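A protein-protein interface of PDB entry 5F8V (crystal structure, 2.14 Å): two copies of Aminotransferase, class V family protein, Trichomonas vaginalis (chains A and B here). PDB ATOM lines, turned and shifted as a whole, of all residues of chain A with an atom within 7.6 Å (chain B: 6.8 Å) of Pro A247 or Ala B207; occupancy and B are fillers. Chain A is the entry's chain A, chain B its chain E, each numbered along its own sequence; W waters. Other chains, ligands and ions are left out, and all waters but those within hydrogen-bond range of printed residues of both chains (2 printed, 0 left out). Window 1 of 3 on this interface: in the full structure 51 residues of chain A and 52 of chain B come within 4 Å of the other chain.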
ATOM      1  N   ILE A  39     -30.948   1.380   6.644  1.00  0.00           N
ATOM      2  CA  ILE A  39     -29.939   1.266   7.714  1.00  0.00           C
ATOM      3  C   ILE A  39     -30.038  -0.045   8.532  1.00  0.00           C
ATOM      4  O   ILE A  39     -29.036  -0.495   9.089  1.00  0.00           O
ATOM      5  CB  ILE A  39     -30.003   2.497   8.664  1.00  0.00           C
ATOM      6  CG1 ILE A  39     -29.617   3.783   7.914  1.00  0.00           C
ATOM      7  CG2 ILE A  39     -29.083   2.337   9.878  1.00  0.00           C
ATOM      8  CD1 ILE A  39     -29.875   5.060   8.694  1.00  0.00           C
ATOM      9  N   VAL A  41     -31.137  -3.138   7.441  1.00  0.00           N
ATOM     10  CA  VAL A  41     -31.302  -4.284   6.557  1.00  0.00           C
ATOM     11  C   VAL A  41     -30.002  -5.088   6.507  1.00  0.00           C
ATOM     12  O   VAL A  41     -28.923  -4.511   6.432  1.00  0.00           O
ATOM     13  CB  VAL A  41     -31.730  -3.784   5.153  1.00  0.00           C
ATOM     14  CG1 VAL A  41     -31.546  -4.849   4.096  1.00  0.00           C
ATOM     15  CG2 VAL A  41     -33.181  -3.321   5.190  1.00  0.00           C
ATOM     16  N   HIS A  43     -26.995  -7.046   4.960  1.00  0.00           N
ATOM     17  CA  HIS A  43     -26.251  -7.062   3.701  1.00  0.00           C
ATOM     18  C   HIS A  43     -26.289  -8.419   2.974  1.00  0.00           C
ATOM     19  O   HIS A  43     -26.112  -8.475   1.758  1.00  0.00           O
ATOM     20  CB  HIS A  43     -24.805  -6.569   3.918  1.00  0.00           C
ATOM     21  CG  HIS A  43     -23.942  -7.493   4.724  1.00  0.00           C
ATOM     22  ND1 HIS A  43     -24.079  -7.657   6.088  1.00  0.00           N
ATOM     23  CD2 HIS A  43     -22.896  -8.272   4.360  1.00  0.00           C
ATOM     24  CE1 HIS A  43     -23.169  -8.507   6.526  1.00  0.00           C
ATOM     25  NE2 HIS A  43     -22.440  -8.896   5.498  1.00  0.00           N
ATOM     26  N   TRP A  48     -30.945  -5.980   0.130  1.00  0.00           N
ATOM     27  CA  TRP A  48     -29.676  -5.257   0.004  1.00  0.00           C
ATOM     28  C   TRP A  48     -28.870  -5.692  -1.229  1.00  0.00           C
ATOM     29  O   TRP A  48     -28.363  -4.851  -1.971  1.00  0.00           O
ATOM     30  CB  TRP A  48     -28.775  -5.333   1.254  1.00  0.00           C
ATOM     31  CG  TRP A  48     -27.539  -4.572   0.930  1.00  0.00           C
ATOM     32  CD1 TRP A  48     -26.294  -5.077   0.667  1.00  0.00           C
ATOM     33  CD2 TRP A  48     -27.476  -3.180   0.643  1.00  0.00           C
ATOM     34  NE1 TRP A  48     -25.442  -4.068   0.293  1.00  0.00           N
ATOM     35  CE2 TRP A  48     -26.143  -2.890   0.264  1.00  0.00           C
ATOM     36  CE3 TRP A  48     -28.413  -2.134   0.691  1.00  0.00           C
ATOM     37  CZ2 TRP A  48     -25.721  -1.595  -0.043  1.00  0.00           C
ATOM     38  CZ3 TRP A  48     -27.996  -0.849   0.377  1.00  0.00           C
ATOM     39  CH2 TRP A  48     -26.657  -0.594   0.015  1.00  0.00           C
ATOM     40  N   GLN A  52     -27.372  -3.033  -4.120  1.00  0.00           N
ATOM     41  CA  GLN A  52     -25.953  -2.865  -4.426  1.00  0.00           C
ATOM     42  C   GLN A  52     -25.631  -3.281  -5.846  1.00  0.00           C
ATOM     43  O   GLN A  52     -24.833  -2.634  -6.510  1.00  0.00           O
ATOM     44  CB  GLN A  52     -25.081  -3.635  -3.450  1.00  0.00           C
ATOM     45  CG  GLN A  52     -23.601  -3.343  -3.656  1.00  0.00           C
ATOM     46  CD  GLN A  52     -22.742  -3.833  -2.516  1.00  0.00           C
ATOM     47  OE1 GLN A  52     -23.078  -3.642  -1.351  1.00  0.00           O
ATOM     48  NE2 GLN A  52     -21.604  -4.434  -2.847  1.00  0.00           N
ATOM     49  N   PHE A  73     -17.331  -0.630  -4.507  1.00  0.00           N
ATOM     50  CA  PHE A  73     -17.689   0.297  -3.444  1.00  0.00           C
ATOM     51  C   PHE A  73     -16.949  -0.212  -2.227  1.00  0.00           C
ATOM     52  O   PHE A  73     -17.116  -1.380  -1.854  1.00  0.00           O
ATOM     53  CB  PHE A  73     -19.190   0.264  -3.163  1.00  0.00           C
ATOM     54  CG  PHE A  73     -20.029   0.792  -4.287  1.00  0.00           C
ATOM     55  CD1 PHE A  73     -20.158   2.161  -4.485  1.00  0.00           C
ATOM     56  CD2 PHE A  73     -20.700  -0.076  -5.148  1.00  0.00           C
ATOM     57  CE1 PHE A  73     -20.937   2.658  -5.522  1.00  0.00           C
ATOM     58  CE2 PHE A  73     -21.476   0.419  -6.190  1.00  0.00           C
ATOM     59  CZ  PHE A  73     -21.596   1.783  -6.378  1.00  0.00           C
ATOM     60  N   VAL A  74     -16.141   0.646  -1.609  1.00  0.00           N
ATOM     61  CA  VAL A  74     -15.351   0.264  -0.427  1.00  0.00           C
ATOM     62  C   VAL A  74     -15.501   1.245   0.728  1.00  0.00           C
ATOM     63  O   VAL A  74     -15.838   2.413   0.528  1.00  0.00           O
ATOM     64  CB  VAL A  74     -13.854   0.096  -0.775  1.00  0.00           C
ATOM     65  CG1 VAL A  74     -13.672  -1.156  -1.620  1.00  0.00           C
ATOM     66  CG2 VAL A  74     -13.293   1.325  -1.502  1.00  0.00           C
ATOM     67  N   ALA A  75     -15.287   0.747   1.943  1.00  0.00           N
ATOM     68  CA  ALA A  75     -15.217   1.595   3.126  1.00  0.00           C
ATOM     69  C   ALA A  75     -13.931   2.403   3.040  1.00  0.00           C
ATOM     70  O   ALA A  75     -12.949   1.935   2.479  1.00  0.00           O
ATOM     71  CB  ALA A  75     -15.226   0.755   4.393  1.00  0.00           C
ATOM     72  N   GLY A  76     -13.947   3.613   3.585  1.00  0.00           N
ATOM     73  CA  GLY A  76     -12.744   4.456   3.644  1.00  0.00           C
ATOM     74  C   GLY A  76     -12.674   5.503   2.540  1.00  0.00           C
ATOM     75  O   GLY A  76     -13.127   5.277   1.420  1.00  0.00           O
ATOM     76  N   LEU A 206     -22.002  10.486   0.779  1.00  0.00           N
ATOM     77  CA  LEU A 206     -21.519  10.366   2.160  1.00  0.00           C
ATOM     78  C   LEU A 206     -20.037  10.174   2.229  1.00  0.00           C
ATOM     79  O   LEU A 206     -19.486   9.368   1.480  1.00  0.00           O
ATOM     80  CB  LEU A 206     -22.169   9.189   2.882  1.00  0.00           C
ATOM     81  CG  LEU A 206     -23.458   9.497   3.630  1.00  0.00           C
ATOM     82  CD1 LEU A 206     -24.653   9.565   2.688  1.00  0.00           C
ATOM     83  CD2 LEU A 206     -23.661   8.441   4.704  1.00  0.00           C
ATOM     84  N   ALA A 207     -19.401  10.878   3.163  1.00  0.00           N
ATOM     85  CA  ALA A 207     -18.021  10.591   3.528  1.00  0.00           C
ATOM     86  C   ALA A 207     -17.952   9.228   4.207  1.00  0.00           C
ATOM     87  O   ALA A 207     -18.914   8.800   4.845  1.00  0.00           O
ATOM     88  CB  ALA A 207     -17.476  11.664   4.454  1.00  0.00           C
ATOM     89  N   GLY A 208     -16.807   8.574   4.065  1.00  0.00           N
ATOM     90  CA  GLY A 208     -16.574   7.235   4.606  1.00  0.00           C
ATOM     91  C   GLY A 208     -16.523   6.141   3.549  1.00  0.00           C
ATOM     92  O   GLY A 208     -16.209   4.994   3.883  1.00  0.00           O
ATOM     93  N   MET A 209     -16.818   6.490   2.291  1.00  0.00           N
ATOM     94  CA  MET A 209     -16.917   5.525   1.196  1.00  0.00           C
ATOM     95  C   MET A 209     -16.231   6.039  -0.067  1.00  0.00           C
ATOM     96  O   MET A 209     -16.282   7.236  -0.366  1.00  0.00           O
ATOM     97  CB  MET A 209     -18.392   5.224   0.889  1.00  0.00           C
ATOM     98  CG  MET A 209     -18.635   4.159  -0.183  1.00  0.00           C
ATOM     99  SD  MET A 209     -18.774   4.790  -1.869  1.00  0.00           S
ATOM    100  CE  MET A 209     -20.452   5.411  -1.820  1.00  0.00           C
ATOM    101  N   SER A 210     -15.608   5.117  -0.804  1.00  0.00           N
ATOM    102  CA  SER A 210     -14.973   5.413  -2.089  1.00  0.00           C
ATOM    103  C   SER A 210     -15.420   4.423  -3.161  1.00  0.00           C
ATOM    104  O   SER A 210     -15.719   3.257  -2.865  1.00  0.00           O
ATOM    105  CB  SER A 210     -13.444   5.343  -1.979  1.00  0.00           C
ATOM    106  OG  SER A 210     -12.928   6.250  -1.021  1.00  0.00           O
ATOM    107  N   CYS A 241     -17.707  -7.030  -3.246  1.00  0.00           N
ATOM    108  CA  CYS A 241     -17.602  -5.975  -2.223  1.00  0.00           C
ATOM    109  C   CYS A 241     -18.349  -6.250  -0.917  1.00  0.00           C
ATOM    110  O   CYS A 241     -18.682  -5.319  -0.178  1.00  0.00           O
ATOM    111  CB  CYS A 241     -18.015  -4.618  -2.795  1.00  0.00           C
ATOM    112  SG  CYS A 241     -16.870  -4.054  -4.047  1.00  0.00           S
ATOM    113  N   ASN A 244     -16.812  -8.308   3.890  1.00  0.00           N
ATOM    114  CA  ASN A 244     -17.390  -7.937   5.174  1.00  0.00           C
ATOM    115  C   ASN A 244     -18.555  -6.997   4.883  1.00  0.00           C
ATOM    116  O   ASN A 244     -18.973  -6.880   3.729  1.00  0.00           O
ATOM    117  CB  ASN A 244     -16.316  -7.322   6.088  1.00  0.00           C
ATOM    118  CG  ASN A 244     -15.854  -5.944   5.628  1.00  0.00           C
ATOM    119  OD1 ASN A 244     -15.703  -5.681   4.430  1.00  0.00           O
ATOM    120  ND2 ASN A 244     -15.617  -5.058   6.589  1.00  0.00           N
ATOM    121  N   THR A 245     -19.098  -6.347   5.908  1.00  0.00           N
ATOM    122  CA  THR A 245     -20.258  -5.491   5.712  1.00  0.00           C
ATOM    123  C   THR A 245     -19.871  -4.209   4.956  1.00  0.00           C
ATOM    124  O   THR A 245     -19.022  -3.450   5.421  1.00  0.00           O
ATOM    125  CB  THR A 245     -20.925  -5.121   7.048  1.00  0.00           C
ATOM    126  OG1 THR A 245     -20.983  -6.279   7.891  1.00  0.00           O
ATOM    127  CG2 THR A 245     -22.341  -4.598   6.814  1.00  0.00           C
ATOM    128  N   PRO A 246     -20.497  -3.967   3.787  1.00  0.00           N
ATOM    129  CA  PRO A 246     -20.224  -2.742   3.035  1.00  0.00           C
ATOM    130  C   PRO A 246     -20.926  -1.539   3.674  1.00  0.00           C
ATOM    131  O   PRO A 246     -21.869  -1.726   4.441  1.00  0.00           O
ATOM    132  CB  PRO A 246     -20.829  -3.053   1.669  1.00  0.00           C
ATOM    133  CG  PRO A 246     -21.998  -3.906   1.987  1.00  0.00           C
ATOM    134  CD  PRO A 246     -21.565  -4.764   3.144  1.00  0.00           C
ATOM    135  N   PRO A 247     -20.485  -0.309   3.365  1.00  0.00           N
ATOM    136  CA  PRO A 247     -21.136   0.871   3.951  1.00  0.00           C
ATOM    137  C   PRO A 247     -22.476   1.144   3.275  1.00  0.00           C
ATOM    138  O   PRO A 247     -22.568   1.979   2.379  1.00  0.00           O
ATOM    139  CB  PRO A 247     -20.116   1.984   3.703  1.00  0.00           C
ATOM    140  CG  PRO A 247     -19.410   1.566   2.452  1.00  0.00           C
ATOM    141  CD  PRO A 247     -19.369   0.060   2.479  1.00  0.00           C
ATOM    142  N   THR A 248     -23.503   0.422   3.721  1.00  0.00           N
ATOM    143  CA  THR A 248     -24.759   0.291   2.971  1.00  0.00           C
ATOM    144  C   THR A 248     -25.486   1.617   2.742  1.00  0.00           C
ATOM    145  O   THR A 248     -25.924   1.905   1.621  1.00  0.00           O
ATOM    146  CB  THR A 248     -25.717  -0.726   3.639  1.00  0.00           C
ATOM    147  OG1 THR A 248     -25.881  -0.399   5.015  1.00  0.00           O
ATOM    148  CG2 THR A 248     -25.168  -2.141   3.551  1.00  0.00           C
ATOM    149  N   PHE A 249     -25.596   2.445   3.776  1.00  0.00           N
ATOM    150  CA  PHE A 249     -26.281   3.729   3.614  1.00  0.00           C
ATOM    151  C   PHE A 249     -25.583   4.631   2.600  1.00  0.00           C
ATOM    152  O   PHE A 249     -26.246   5.337   1.839  1.00  0.00           O
ATOM    153  CB  PHE A 249     -26.465   4.453   4.952  1.00  0.00           C
ATOM    154  CG  PHE A 249     -27.437   5.606   4.882  1.00  0.00           C
ATOM    155  CD1 PHE A 249     -26.987   6.910   4.692  1.00  0.00           C
ATOM    156  CD2 PHE A 249     -28.801   5.387   4.982  1.00  0.00           C
ATOM    157  CE1 PHE A 249     -27.880   7.970   4.618  1.00  0.00           C
ATOM    158  CE2 PHE A 249     -29.706   6.442   4.911  1.00  0.00           C
ATOM    159  CZ  PHE A 249     -29.247   7.735   4.724  1.00  0.00           C
ATOM    160  N   ALA A 250     -24.252   4.590   2.562  1.00  0.00           N
ATOM    161  CA  ALA A 250     -23.494   5.381   1.597  1.00  0.00           C
ATOM    162  C   ALA A 250     -23.751   4.924   0.158  1.00  0.00           C
ATOM    163  O   ALA A 250     -23.865   5.754  -0.755  1.00  0.00           O
ATOM    164  CB  ALA A 250     -22.011   5.325   1.922  1.00  0.00           C
ATOM    165  N   ILE A 251     -23.862   3.607  -0.038  1.00  0.00           N
ATOM    166  CA  ILE A 251     -24.069   3.034  -1.368  1.00  0.00           C
ATOM    167  C   ILE A 251     -25.481   3.330  -1.854  1.00  0.00           C
ATOM    168  O   ILE A 251     -25.666   3.779  -2.984  1.00  0.00           O
ATOM    169  CB  ILE A 251     -23.785   1.508  -1.381  1.00  0.00           C
ATOM    170  CG1 ILE A 251     -22.292   1.251  -1.120  1.00  0.00           C
ATOM    171  CG2 ILE A 251     -24.183   0.878  -2.718  1.00  0.00           C
ATOM    172  CD1 ILE A 251     -22.001  -0.097  -0.497  1.00  0.00           C
ATOM    173  N   TYR A 252     -26.461   3.060  -0.995  1.00  0.00           N
ATOM    174  CA  TYR A 252     -27.866   3.438  -1.220  1.00  0.00           C
ATOM    175  C   TYR A 252     -28.004   4.921  -1.592  1.00  0.00           C
ATOM    176  O   TYR A 252     -28.718   5.265  -2.533  1.00  0.00           O
ATOM    177  CB  TYR A 252     -28.711   3.109   0.036  1.00  0.00           C
ATOM    178  CG  TYR A 252     -29.920   3.990   0.287  1.00  0.00           C
ATOM    179  CD1 TYR A 252     -31.163   3.673  -0.249  1.00  0.00           C
ATOM    180  CD2 TYR A 252     -29.824   5.130   1.090  1.00  0.00           C
ATOM    181  CE1 TYR A 252     -32.268   4.468  -0.006  1.00  0.00           C
ATOM    182  CE2 TYR A 252     -30.923   5.939   1.327  1.00  0.00           C
ATOM    183  CZ  TYR A 252     -32.143   5.606   0.778  1.00  0.00           C
ATOM    184  OH  TYR A 252     -33.231   6.409   1.023  1.00  0.00           O
ATOM    185  N   PHE A 253     -27.336   5.790  -0.840  1.00  0.00           N
ATOM    186  CA  PHE A 253     -27.438   7.223  -1.083  1.00  0.00           C
ATOM    187  C   PHE A 253     -26.708   7.639  -2.359  1.00  0.00           C
ATOM    188  O   PHE A 253     -27.196   8.477  -3.110  1.00  0.00           O
ATOM    189  CB  PHE A 253     -26.964   8.046   0.115  1.00  0.00           C
ATOM    190  CG  PHE A 253     -27.481   9.454   0.097  1.00  0.00           C
ATOM    191  CD1 PHE A 253     -26.681  10.504  -0.342  1.00  0.00           C
ATOM    192  CD2 PHE A 253     -28.791   9.721   0.462  1.00  0.00           C
ATOM    193  CE1 PHE A 253     -27.173  11.800  -0.370  1.00  0.00           C
ATOM    194  CE2 PHE A 253     -29.290  11.012   0.422  1.00  0.00           C
ATOM    195  CZ  PHE A 253     -28.480  12.051   0.005  1.00  0.00           C
ATOM    196  N   PRO B  13     -26.222  -5.416   9.199  1.00  0.00           N
ATOM    197  CA  PRO B  13     -26.734  -4.303  10.015  1.00  0.00           C
ATOM    198  C   PRO B  13     -28.092  -4.617  10.645  1.00  0.00           C
ATOM    199  O   PRO B  13     -28.841  -5.451  10.124  1.00  0.00           O
ATOM    200  CB  PRO B  13     -26.852  -3.161   9.011  1.00  0.00           C
ATOM    201  CG  PRO B  13     -25.801  -3.465   7.998  1.00  0.00           C
ATOM    202  CD  PRO B  13     -25.848  -4.957   7.852  1.00  0.00           C
ATOM    203  N   GLY B  76     -14.205   2.249   8.344  1.00  0.00           N
ATOM    204  CA  GLY B  76     -13.914   0.822   8.237  1.00  0.00           C
ATOM    205  C   GLY B  76     -14.584  -0.018   9.302  1.00  0.00           C
ATOM    206  O   GLY B  76     -14.784   0.418  10.442  1.00  0.00           O
ATOM    207  N   GLY B  77     -14.926  -1.239   8.915  1.00  0.00           N
ATOM    208  CA  GLY B  77     -15.592  -2.186   9.800  1.00  0.00           C
ATOM    209  C   GLY B  77     -14.618  -2.850  10.741  1.00  0.00           C
ATOM    210  O   GLY B  77     -13.432  -2.492  10.801  1.00  0.00           O
ATOM    211  N   CYS B 199     -17.384  -2.438  15.431  1.00  0.00           N
ATOM    212  CA  CYS B 199     -18.075  -1.880  14.279  1.00  0.00           C
ATOM    213  C   CYS B 199     -19.421  -1.326  14.755  1.00  0.00           C
ATOM    214  O   CYS B 199     -19.952  -1.757  15.775  1.00  0.00           O
ATOM    215  CB  CYS B 199     -18.260  -2.943  13.194  1.00  0.00           C
ATOM    216  SG  CYS B 199     -19.402  -4.273  13.646  1.00  0.00           S
ATOM    217  N   ALA B 200     -19.950  -0.363  14.016  1.00  0.00           N
ATOM    218  CA  ALA B 200     -21.129   0.386  14.443  1.00  0.00           C
ATOM    219  C   ALA B 200     -22.455  -0.322  14.188  1.00  0.00           C
ATOM    220  O   ALA B 200     -23.412  -0.113  14.937  1.00  0.00           O
ATOM    221  CB  ALA B 200     -21.131   1.773  13.814  1.00  0.00           C
ATOM    222  N   GLN B 201     -22.505  -1.180  13.169  1.00  0.00           N
ATOM    223  CA  GLN B 201     -23.792  -1.679  12.627  1.00  0.00           C
ATOM    224  C   GLN B 201     -24.587  -2.706  13.450  1.00  0.00           C
ATOM    225  O   GLN B 201     -25.614  -3.213  12.967  1.00  0.00           O
ATOM    226  CB  GLN B 201     -23.610  -2.215  11.192  1.00  0.00           C
ATOM    227  CG  GLN B 201     -22.828  -3.531  11.045  1.00  0.00           C
ATOM    228  CD  GLN B 201     -21.338  -3.330  10.830  1.00  0.00           C
ATOM    229  OE1 GLN B 201     -20.775  -2.328  11.252  1.00  0.00           O
ATOM    230  NE2 GLN B 201     -20.692  -4.295  10.187  1.00  0.00           N
ATOM    231  N1  LLP B 202     -16.746  -9.200  14.676  1.00  0.00           N
ATOM    232  C2  LLP B 202     -17.928  -9.470  15.290  1.00  0.00           C
ATOM    233  C2' LLP B 202     -17.944  -9.953  16.720  1.00  0.00           C
ATOM    234  C3  LLP B 202     -19.201  -9.303  14.538  1.00  0.00           C
ATOM    235  O3  LLP B 202     -20.411  -9.562  15.104  1.00  0.00           O
ATOM    236  C4  LLP B 202     -19.121  -8.845  13.129  1.00  0.00           C
ATOM    237  C4' LLP B 202     -20.419  -8.658  12.363  1.00  0.00           C
ATOM    238  C5  LLP B 202     -17.756  -8.582  12.582  1.00  0.00           C
ATOM    239  C6  LLP B 202     -16.641  -8.773  13.402  1.00  0.00           C
ATOM    240  C5' LLP B 202     -17.527  -8.110  11.164  1.00  0.00           C
ATOM    241  OP4 LLP B 202     -17.749  -6.709  11.085  1.00  0.00           O
ATOM    242  P   LLP B 202     -17.529  -5.952   9.684  1.00  0.00           P
ATOM    243  OP1 LLP B 202     -16.086  -6.239   9.334  1.00  0.00           O
ATOM    244  OP2 LLP B 202     -18.534  -6.584   8.744  1.00  0.00           O
ATOM    245  OP3 LLP B 202     -17.821  -4.525  10.086  1.00  0.00           O
ATOM    246  N   LLP B 202     -24.132  -3.034  14.660  1.00  0.00           N
ATOM    247  CA  LLP B 202     -24.851  -3.986  15.514  1.00  0.00           C
ATOM    248  CB  LLP B 202     -23.881  -4.982  16.156  1.00  0.00           C
ATOM    249  CG  LLP B 202     -23.721  -6.243  15.300  1.00  0.00           C
ATOM    250  CD  LLP B 202     -22.368  -6.318  14.602  1.00  0.00           C
ATOM    251  CE  LLP B 202     -22.328  -7.448  13.573  1.00  0.00           C
ATOM    252  NZ  LLP B 202     -21.052  -7.455  12.874  1.00  0.00           N
ATOM    253  C   LLP B 202     -25.648  -3.222  16.527  1.00  0.00           C
ATOM    254  O   LLP B 202     -26.866  -3.354  16.566  1.00  0.00           O
ATOM    255  N   GLY B 205     -25.665   1.859  14.910  1.00  0.00           N
ATOM    256  CA  GLY B 205     -26.063   2.503  13.655  1.00  0.00           C
ATOM    257  C   GLY B 205     -25.508   1.960  12.347  1.00  0.00           C
ATOM    258  O   GLY B 205     -25.898   0.877  11.908  1.00  0.00           O
ATOM    259  N   LEU B 206     -24.626   2.731  11.704  1.00  0.00           N
ATOM    260  CA  LEU B 206     -24.254   2.461  10.302  1.00  0.00           C
ATOM    261  C   LEU B 206     -23.085   1.506  10.162  1.00  0.00           C
ATOM    262  O   LEU B 206     -22.207   1.465  11.009  1.00  0.00           O
ATOM    263  CB  LEU B 206     -23.938   3.757   9.554  1.00  0.00           C
ATOM    264  CG  LEU B 206     -25.149   4.467   8.946  1.00  0.00           C
ATOM    265  CD1 LEU B 206     -25.933   5.218  10.009  1.00  0.00           C
ATOM    266  CD2 LEU B 206     -24.705   5.418   7.845  1.00  0.00           C
ATOM    267  N   ALA B 207     -23.081   0.744   9.075  1.00  0.00           N
ATOM    268  CA  ALA B 207     -21.913  -0.040   8.693  1.00  0.00           C
ATOM    269  C   ALA B 207     -20.844   0.887   8.134  1.00  0.00           C
ATOM    270  O   ALA B 207     -21.142   2.005   7.716  1.00  0.00           O
ATOM    271  CB  ALA B 207     -22.291  -1.095   7.672  1.00  0.00           C
ATOM    272  N   GLY B 208     -19.604   0.410   8.134  1.00  0.00           N
ATOM    273  CA  GLY B 208     -18.478   1.152   7.579  1.00  0.00           C
ATOM    274  C   GLY B 208     -17.795   2.087   8.565  1.00  0.00           C
ATOM    275  O   GLY B 208     -16.921   2.848   8.176  1.00  0.00           O
ATOM    276  N   MET B 209     -18.177   2.028   9.839  1.00  0.00           N
ATOM    277  CA  MET B 209     -17.518   2.817  10.881  1.00  0.00           C
ATOM    278  C   MET B 209     -17.337   1.926  12.091  1.00  0.00           C
ATOM    279  O   MET B 209     -18.184   1.067  12.363  1.00  0.00           O
ATOM    280  CB  MET B 209     -18.352   4.054  11.230  1.00  0.00           C
ATOM    281  CG  MET B 209     -17.745   4.975  12.285  1.00  0.00           C
ATOM    282  SD  MET B 209     -18.184   4.556  13.988  1.00  0.00           S
ATOM    283  CE  MET B 209     -19.866   5.154  14.079  1.00  0.00           C
ATOM    284  N   SER B 210     -16.232   2.128  12.805  1.00  0.00           N
ATOM    285  CA  SER B 210     -15.987   1.434  14.068  1.00  0.00           C
ATOM    286  C   SER B 210     -15.535   2.412  15.144  1.00  0.00           C
ATOM    287  O   SER B 210     -14.933   3.445  14.847  1.00  0.00           O
ATOM    288  CB  SER B 210     -14.926   0.348  13.897  1.00  0.00           C
ATOM    289  OG  SER B 210     -15.275  -0.554  12.862  1.00  0.00           O
ATOM    290  N   PRO B 247     -16.186   9.496   8.679  1.00  0.00           N
ATOM    291  CA  PRO B 247     -17.540   9.079   8.266  1.00  0.00           C
ATOM    292  C   PRO B 247     -18.637   9.832   9.037  1.00  0.00           C
ATOM    293  O   PRO B 247     -19.262   9.284   9.957  1.00  0.00           O
ATOM    294  CB  PRO B 247     -17.545   7.573   8.577  1.00  0.00           C
ATOM    295  CG  PRO B 247     -16.611   7.441   9.731  1.00  0.00           C
ATOM    296  CD  PRO B 247     -15.519   8.445   9.472  1.00  0.00           C
ATOM    297  N   ALA B 250     -22.309   8.506   9.966  1.00  0.00           N
ATOM    298  CA  ALA B 250     -22.213   7.419  10.936  1.00  0.00           C
ATOM    299  C   ALA B 250     -21.978   7.903  12.371  1.00  0.00           C
ATOM    300  O   ALA B 250     -22.573   7.371  13.294  1.00  0.00           O
ATOM    301  CB  ALA B 250     -21.129   6.433  10.526  1.00  0.00           C
HETATM  302  O   HOH W   1     -18.654  -2.444   8.237  1.00  0.00           O
HETATM  303  O   HOH W   2     -14.662  -2.291   6.183  1.00  0.00           O
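The side-chain amide nitrogen of Asn A244 sits at hydrogen-bond distance from OP1 of LLP B202, at 3.0 Å. OG1 of Thr A245 lies within hydrogen-bond range of OP2 of LLP B202, at 2.6 Å. The side-chain hydroxyl of Thr A245 sits at hydrogen-bond distance from the side-chain amide nitrogen of Gln B201 (3.0 Å).
The backbone NH (N) of Gln B201 lies within hydrogen-bond range of the backbone carbonyl oxygen (O) of Leu B206, at 3.4 Å. OE1 of Gln B201 sits close to SG of Cys B199 (3.4 Å). The side-chain sulfur (SG) of Cys B199 is in hydrogen-bond range of NZ of LLP B202. The side-chain amide nitrogen (NE2) of Gln B201 lies within hydrogen-bond range of OP3 of LLP B202 (2.9 Å).
Pro B13 touches Ile A39. Pro B13 touches Val A41 (CD to O, 3.4 Å). His A43 touches Pro B13. Ala A207 touches Pro B247 (O to CA, 3.7 Å). Pro B13 touches Thr A245 (CD to CG2, 3.7 Å). Thr A245 touches Ala B207 (CG2 to CB, 3.6 Å). CB of Ala B207 touches O of Pro A246 (3.3 Å). CA of Pro A247 touches O of Ala B207, at 3.9 Å. Leu B206 touches Phe A249.
Ala B207 touches three residues of chain A. Of the printed residues of chain A, LLP B202 touches Asn A244 and Thr A245. Printed residues of chain B within 4 Å of His A43: Pro B13 (3.7 Å). Of the printed residues of chain B, Ala A207 touches Pro B247 (3.7 Å). Printed residues of chain B within 4 Å of Asn A244: LLP B202. Trp A48 touches none of the printed residues of chain B. Ala B200 touches none of the printed residues of chain A. The nearest printed residue of chain A that does not touch LLP B202 is His A43 (5.5 Å).
Of the 25 printed residues of chain A, 9 touch a printed residue of chain B. Of the 15 printed residues of chain B, 6 touch a printed residue of chain A. Hydrophobic or aromatic side chains of chain B that line the printed part of chain A: Pro B13, Leu B206 and Ala B207. Along chain B the printed residues that touch a printed residue of chain A span positions 13 to 247. Among the printed residues, no Asp or Glu carboxylate lies within 4 Å of a Lys or Arg side-chain nitrogen of the other chain.
Ala A207 touches Pro B247, and with the chains exchanged Pro A247 touches Ala B207. Of the 12 pairs that touch across the chains among the printed residues, 2 have their exchanged pair printed and touching as well.
Water W1 lies within hydrogen-bond range of OP3 of LLP B202 (2.9 Å), the backbone NH (N) of Gly B208 (3.0 Å), the backbone carbonyl oxygen (O) of Thr A245 (3.0 Å) and the side-chain amide nitrogen (NE2) of Gln B201 (3.4 Å). Water W2 bridges the backbone NH (N) of Gly B77 (2.9 Å) and the side-chain amide nitrogen (ND2) of Asn A244 (3.0 Å).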
